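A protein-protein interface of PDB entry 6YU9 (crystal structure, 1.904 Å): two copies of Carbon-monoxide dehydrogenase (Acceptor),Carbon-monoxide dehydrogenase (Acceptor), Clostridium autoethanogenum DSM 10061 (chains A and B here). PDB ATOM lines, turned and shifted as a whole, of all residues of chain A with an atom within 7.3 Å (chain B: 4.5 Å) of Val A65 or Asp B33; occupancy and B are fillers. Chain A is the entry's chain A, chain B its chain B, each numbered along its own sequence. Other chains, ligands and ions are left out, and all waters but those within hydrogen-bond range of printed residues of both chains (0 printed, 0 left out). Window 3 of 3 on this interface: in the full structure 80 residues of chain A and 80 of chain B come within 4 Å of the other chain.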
ATOM      1  N   PHE A  40      14.400  15.300 -15.689  1.00  0.00           N
ATOM      2  CA  PHE A  40      15.371  16.195 -15.047  1.00  0.00           C
ATOM      3  C   PHE A  40      14.939  16.459 -13.593  1.00  0.00           C
ATOM      4  O   PHE A  40      15.706  16.158 -12.685  1.00  0.00           O
ATOM      5  CB  PHE A  40      15.465  17.515 -15.816  1.00  0.00           C
ATOM      6  CG  PHE A  40      16.113  17.351 -17.161  1.00  0.00           C
ATOM      7  CD1 PHE A  40      17.479  17.131 -17.266  1.00  0.00           C
ATOM      8  CD2 PHE A  40      15.368  17.469 -18.330  1.00  0.00           C
ATOM      9  CE1 PHE A  40      18.094  17.002 -18.521  1.00  0.00           C
ATOM     10  CE2 PHE A  40      15.991  17.388 -19.585  1.00  0.00           C
ATOM     11  CZ  PHE A  40      17.351  17.150 -19.670  1.00  0.00           C
ATOM     12  N   ARG A  56      19.184  23.031 -16.514  1.00  0.00           N
ATOM     13  CA  ARG A  56      19.062  21.590 -16.372  1.00  0.00           C
ATOM     14  C   ARG A  56      20.370  21.025 -16.842  1.00  0.00           C
ATOM     15  O   ARG A  56      20.945  21.548 -17.791  1.00  0.00           O
ATOM     16  CB  ARG A  56      17.871  20.966 -17.122  1.00  0.00           C
ATOM     17  CG  ARG A  56      17.665  21.435 -18.534  1.00  0.00           C
ATOM     18  CD  ARG A  56      16.390  20.842 -19.109  1.00  0.00           C
ATOM     19  NE  ARG A  56      15.956  21.560 -20.305  1.00  0.00           N
ATOM     20  CZ  ARG A  56      14.750  21.447 -20.862  1.00  0.00           C
ATOM     21  NH1 ARG A  56      13.835  20.635 -20.342  1.00  0.00           N
ATOM     22  NH2 ARG A  56      14.450  22.158 -21.949  1.00  0.00           N
ATOM     23  N   VAL A  57      20.933  20.101 -16.063  1.00  0.00           N
ATOM     24  CA  VAL A  57      22.203  19.476 -16.374  1.00  0.00           C
ATOM     25  C   VAL A  57      21.971  17.977 -16.551  1.00  0.00           C
ATOM     26  O   VAL A  57      20.913  17.481 -16.199  1.00  0.00           O
ATOM     27  CB  VAL A  57      23.325  19.805 -15.352  1.00  0.00           C
ATOM     28  CG1 VAL A  57      23.496  21.313 -15.202  1.00  0.00           C
ATOM     29  CG2 VAL A  57      23.074  19.157 -13.986  1.00  0.00           C
ATOM     30  N   SER A  58      22.933  17.281 -17.191  1.00  0.00           N
ATOM     31  CA  SER A  58      22.821  15.873 -17.469  1.00  0.00           C
ATOM     32  C   SER A  58      22.779  15.041 -16.181  1.00  0.00           C
ATOM     33  O   SER A  58      23.641  15.214 -15.334  1.00  0.00           O
ATOM     34  CB  SER A  58      24.001  15.429 -18.333  1.00  0.00           C
ATOM     35  OG  SER A  58      24.122  14.016 -18.456  1.00  0.00           O
ATOM     36  N   PRO A  59      21.830  14.105 -16.030  1.00  0.00           N
ATOM     37  CA  PRO A  59      21.857  13.195 -14.879  1.00  0.00           C
ATOM     38  C   PRO A  59      22.800  12.019 -15.118  1.00  0.00           C
ATOM     39  O   PRO A  59      22.862  11.081 -14.314  1.00  0.00           O
ATOM     40  CB  PRO A  59      20.421  12.703 -14.795  1.00  0.00           C
ATOM     41  CG  PRO A  59      19.924  12.753 -16.182  1.00  0.00           C
ATOM     42  CD  PRO A  59      20.744  13.759 -16.955  1.00  0.00           C
ATOM     43  N   VAL A  60      23.528  12.043 -16.247  1.00  0.00           N
ATOM     44  CA  VAL A  60      24.531  11.031 -16.574  1.00  0.00           C
ATOM     45  C   VAL A  60      25.868  11.728 -16.615  1.00  0.00           C
ATOM     46  O   VAL A  60      26.091  12.532 -17.516  1.00  0.00           O
ATOM     47  CB  VAL A  60      24.254  10.364 -17.935  1.00  0.00           C
ATOM     48  CG1 VAL A  60      25.386   9.401 -18.311  1.00  0.00           C
ATOM     49  CG2 VAL A  60      22.916   9.640 -17.918  1.00  0.00           C
ATOM     50  N   LYS A  63      28.397  13.205 -19.846  1.00  0.00           N
ATOM     51  CA  LYS A  63      27.623  13.425 -21.060  1.00  0.00           C
ATOM     52  C   LYS A  63      26.738  14.659 -20.909  1.00  0.00           C
ATOM     53  O   LYS A  63      26.414  15.081 -19.801  1.00  0.00           O
ATOM     54  CB  LYS A  63      26.759  12.202 -21.363  1.00  0.00           C
ATOM     55  CG  LYS A  63      27.501  10.876 -21.350  1.00  0.00           C
ATOM     56  CD  LYS A  63      28.525  10.777 -22.436  1.00  0.00           C
ATOM     57  CE  LYS A  63      28.965   9.363 -22.672  1.00  0.00           C
ATOM     58  NZ  LYS A  63      30.322   9.098 -22.127  1.00  0.00           N
ATOM     59  N   GLY A  64      26.370  15.227 -22.039  1.00  0.00           N
ATOM     60  CA  GLY A  64      25.483  16.380 -22.102  1.00  0.00           C
ATOM     61  C   GLY A  64      25.975  17.626 -21.406  1.00  0.00           C
ATOM     62  O   GLY A  64      27.171  17.809 -21.178  1.00  0.00           O
ATOM     63  N   VAL A  65      25.035  18.501 -21.088  1.00  0.00           N
ATOM     64  CA  VAL A  65      25.340  19.756 -20.366  1.00  0.00           C
ATOM     65  C   VAL A  65      25.649  19.447 -18.901  1.00  0.00           C
ATOM     66  O   VAL A  65      24.860  18.787 -18.250  1.00  0.00           O
ATOM     67  CB  VAL A  65      24.184  20.727 -20.471  1.00  0.00           C
ATOM     68  CG1 VAL A  65      24.515  22.023 -19.728  1.00  0.00           C
ATOM     69  CG2 VAL A  65      23.852  20.996 -21.933  1.00  0.00           C
ATOM     70  N   GLU A  66      26.839  19.823 -18.422  1.00  0.00           N
ATOM     71  CA  GLU A  66      27.276  19.408 -17.093  1.00  0.00           C
ATOM     72  C   GLU A  66      27.170  20.482 -16.018  1.00  0.00           C
ATOM     73  O   GLU A  66      27.158  20.132 -14.827  1.00  0.00           O
ATOM     74  CB  GLU A  66      28.714  18.876 -17.174  1.00  0.00           C
ATOM     75  CG  GLU A  66      28.841  17.672 -18.108  1.00  0.00           C
ATOM     76  CD  GLU A  66      28.959  16.306 -17.454  1.00  0.00           C
ATOM     77  OE1 GLU A  66      30.098  15.799 -17.306  1.00  0.00           O
ATOM     78  OE2 GLU A  66      27.902  15.729 -17.109  1.00  0.00           O
ATOM     79  N   ARG A  67      27.142  21.772 -16.410  1.00  0.00           N
ATOM     80  CA  ARG A  67      27.067  22.834 -15.404  1.00  0.00           C
ATOM     81  C   ARG A  67      25.942  23.820 -15.689  1.00  0.00           C
ATOM     82  O   ARG A  67      25.564  24.004 -16.850  1.00  0.00           O
ATOM     83  CB  ARG A  67      28.411  23.561 -15.270  1.00  0.00           C
ATOM     84  CG  ARG A  67      29.484  22.630 -14.707  1.00  0.00           C
ATOM     85  CD  ARG A  67      30.872  23.207 -14.741  1.00  0.00           C
ATOM     86  NE  ARG A  67      31.203  23.827 -13.455  1.00  0.00           N
ATOM     87  CZ  ARG A  67      32.101  23.378 -12.573  1.00  0.00           C
ATOM     88  NH1 ARG A  67      32.816  22.284 -12.836  1.00  0.00           N
ATOM     89  NH2 ARG A  67      32.309  24.037 -11.433  1.00  0.00           N
ATOM     90  N   GLY A  68      25.383  24.389 -14.619  1.00  0.00           N
ATOM     91  CA  GLY A  68      24.363  25.429 -14.705  1.00  0.00           C
ATOM     92  C   GLY A  68      25.018  26.723 -15.134  1.00  0.00           C
ATOM     93  O   GLY A  68      26.243  26.836 -15.128  1.00  0.00           O
ATOM     94  N   ILE A  69      24.232  27.725 -15.543  1.00  0.00           N
ATOM     95  CA  ILE A  69      24.823  28.965 -16.087  1.00  0.00           C
ATOM     96  C   ILE A  69      25.813  29.610 -15.126  1.00  0.00           C
ATOM     97  O   ILE A  69      26.830  30.141 -15.564  1.00  0.00           O
ATOM     98  CB  ILE A  69      23.700  29.926 -16.502  1.00  0.00           C
ATOM     99  CG1 ILE A  69      22.906  29.264 -17.686  1.00  0.00           C
ATOM    100  CG2 ILE A  69      24.249  31.339 -16.831  1.00  0.00           C
ATOM    101  CD1 ILE A  69      21.612  29.848 -17.982  1.00  0.00           C
ATOM    102  N   ALA A  74      25.814  19.083 -11.156  1.00  0.00           N
ATOM    103  CA  ALA A  74      24.640  18.284 -10.872  1.00  0.00           C
ATOM    104  C   ALA A  74      24.544  18.011  -9.378  1.00  0.00           C
ATOM    105  O   ALA A  74      23.443  18.053  -8.826  1.00  0.00           O
ATOM    106  CB  ALA A  74      24.731  16.952 -11.610  1.00  0.00           C
ATOM    107  N   ASP B  29      29.250  31.416 -22.155  1.00  0.00           N
ATOM    108  CA  ASP B  29      29.342  30.136 -22.867  1.00  0.00           C
ATOM    109  C   ASP B  29      28.335  29.139 -22.280  1.00  0.00           C
ATOM    110  O   ASP B  29      27.692  28.411 -23.027  1.00  0.00           O
ATOM    111  CB  ASP B  29      30.758  29.567 -22.746  1.00  0.00           C
ATOM    112  CG  ASP B  29      31.816  30.472 -23.338  1.00  0.00           C
ATOM    113  OD1 ASP B  29      31.533  31.123 -24.370  1.00  0.00           O
ATOM    114  OD2 ASP B  29      32.923  30.541 -22.768  1.00  0.00           O
ATOM    115  N   ARG B  30      28.216  29.072 -20.936  1.00  0.00           N
ATOM    116  CA  ARG B  30      27.273  28.148 -20.278  1.00  0.00           C
ATOM    117  C   ARG B  30      25.812  28.558 -20.535  1.00  0.00           C
ATOM    118  O   ARG B  30      24.934  27.709 -20.587  1.00  0.00           O
ATOM    119  CB  ARG B  30      27.569  28.096 -18.780  1.00  0.00           C
ATOM    120  CG  ARG B  30      28.948  27.476 -18.478  1.00  0.00           C
ATOM    121  CD  ARG B  30      29.142  27.207 -17.013  1.00  0.00           C
ATOM    122  NE  ARG B  30      29.078  28.471 -16.277  1.00  0.00           N
ATOM    123  CZ  ARG B  30      30.137  29.214 -15.969  1.00  0.00           C
ATOM    124  NH1 ARG B  30      31.364  28.805 -16.280  1.00  0.00           N
ATOM    125  NH2 ARG B  30      29.968  30.386 -15.333  1.00  0.00           N
ATOM    126  N   LYS B  31      25.558  29.854 -20.725  1.00  0.00           N
ATOM    127  CA  LYS B  31      24.240  30.350 -21.115  1.00  0.00           C
ATOM    128  C   LYS B  31      23.898  29.770 -22.503  1.00  0.00           C
ATOM    129  O   LYS B  31      22.825  29.223 -22.702  1.00  0.00           O
ATOM    130  CB  LYS B  31      24.250  31.880 -21.186  1.00  0.00           C
ATOM    131  CG  LYS B  31      23.016  32.458 -21.856  1.00  0.00           C
ATOM    132  CD  LYS B  31      21.753  32.183 -21.058  1.00  0.00           C
ATOM    133  CE  LYS B  31      20.610  33.010 -21.577  1.00  0.00           C
ATOM    134  NZ  LYS B  31      19.600  32.198 -22.278  1.00  0.00           N
ATOM    135  N   ALA B  32      24.807  29.896 -23.460  1.00  0.00           N
ATOM    136  CA  ALA B  32      24.611  29.341 -24.793  1.00  0.00           C
ATOM    137  C   ALA B  32      24.468  27.780 -24.703  1.00  0.00           C
ATOM    138  O   ALA B  32      23.643  27.204 -25.418  1.00  0.00           O
ATOM    139  CB  ALA B  32      25.786  29.708 -25.669  1.00  0.00           C
ATOM    140  N   ASP B  33      25.228  27.091 -23.813  1.00  0.00           N
ATOM    141  CA  ASP B  33      25.121  25.619 -23.709  1.00  0.00           C
ATOM    142  C   ASP B  33      23.748  25.200 -23.192  1.00  0.00           C
ATOM    143  O   ASP B  33      23.319  24.079 -23.448  1.00  0.00           O
ATOM    144  CB  ASP B  33      26.222  25.029 -22.803  1.00  0.00           C
ATOM    145  CG  ASP B  33      27.645  25.148 -23.344  1.00  0.00           C
ATOM    146  OD1 ASP B  33      27.799  25.527 -24.539  1.00  0.00           O
ATOM    147  OD2 ASP B  33      28.616  24.919 -22.551  1.00  0.00           O
ATOM    148  N   MET B  34      23.065  26.075 -22.453  1.00  0.00           N
ATOM    149  CA  MET B  34      21.755  25.763 -21.900  1.00  0.00           C
ATOM    150  C   MET B  34      20.656  25.782 -22.993  1.00  0.00           C
ATOM    151  O   MET B  34      19.543  25.336 -22.744  1.00  0.00           O
ATOM    152  CB  MET B  34      21.435  26.759 -20.753  1.00  0.00           C
ATOM    153  CG  MET B  34      20.509  26.207 -19.677  1.00  0.00           C
ATOM    154  SD  MET B  34      21.019  24.600 -18.985  1.00  0.00           S
ATOM    155  CE  MET B  34      22.436  25.058 -18.067  1.00  0.00           C
ATOM    156  N   LYS B  35      20.970  26.296 -24.199  1.00  0.00           N
ATOM    157  CA  LYS B  35      20.043  26.374 -25.330  1.00  0.00           C
ATOM    158  C   LYS B  35      18.669  26.908 -24.913  1.00  0.00           C
ATOM    159  O   LYS B  35      18.620  27.832 -24.120  1.00  0.00           O
ATOM    160  CB  LYS B  35      19.959  25.025 -26.075  1.00  0.00           C
ATOM    161  CG  LYS B  35      21.309  24.409 -26.406  1.00  0.00           C
ATOM    162  CD  LYS B  35      21.935  25.004 -27.647  1.00  0.00           C
ATOM    163  CE  LYS B  35      23.092  24.198 -28.186  1.00  0.00           C
ATOM    164  NZ  LYS B  35      22.838  22.716 -28.124  1.00  0.00           N
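Of the printed residues of chain B, Val A65 touches Asp B33 (3.5 Å). Glu A66 touches none of the printed residues of chain B. Of the printed residues of chain B, Gly A68 touches Arg B30 (3.5 Å) and Met B34 (3.9 Å). Printed residues of chain B within 4 Å of Ile A69: Arg B30 (2.9 Å) and Lys B31 (3.8 Å). Printed residues of chain A within 4 Å of Arg B30: Gly A68 (3.5 Å) and Ile A69 (2.9 Å). Of chain A, only Val A65 comes within 4 Å of Asp B33. The nearest residue of chain B that does not touch Val A65 is Met B34 (4.04 Å). The nearest residue of chain A that does not touch Asp B33 is Arg A67 (6.1 Å). The nearest printed residue of chain A that does not touch Arg B30 is Arg A67 (4.1 Å).
Among the printed residues, merely in contact across the chains: Val A65 with Asp B33, Arg A67 with Met B34, Gly A68 with Met B34 and Ile A69 with Lys B31.
The backbone carbonyl oxygen (O) of Ile A69 sits at hydrogen-bond distance from the guanidinium group (NE) of Arg B30 (2.9 Å). The backbone carbonyl oxygen (O) of Gly A68 sits at hydrogen-bond distance from the guanidinium group (NE) of Arg B30 (3.5 Å). The backbone NH of Arg A56 is in hydrogen-bond range of the side-chain sulfur of Met B34 (3.5 Å).
Of the 7 printed residues of chain B, 4 touch a printed residue of chain A. Hydrophobic or aromatic side chains of chain B that line the printed part of chain A: Met B34. Along chain B the printed residues that touch a printed residue of chain A span positions 30 to 34. Hydrophobic or aromatic side chains of chain A within 4 Å of the printed part of chain B: Val A65 and Ile A69.
No position is printed for both chains. Of the 7 pairs that touch across the chains among the printed residues, none has its exchanged pair printed and touching as well.
O of Val A65 sits at hydrogen-bond distance from N of Ser A58 (2.7 Å).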
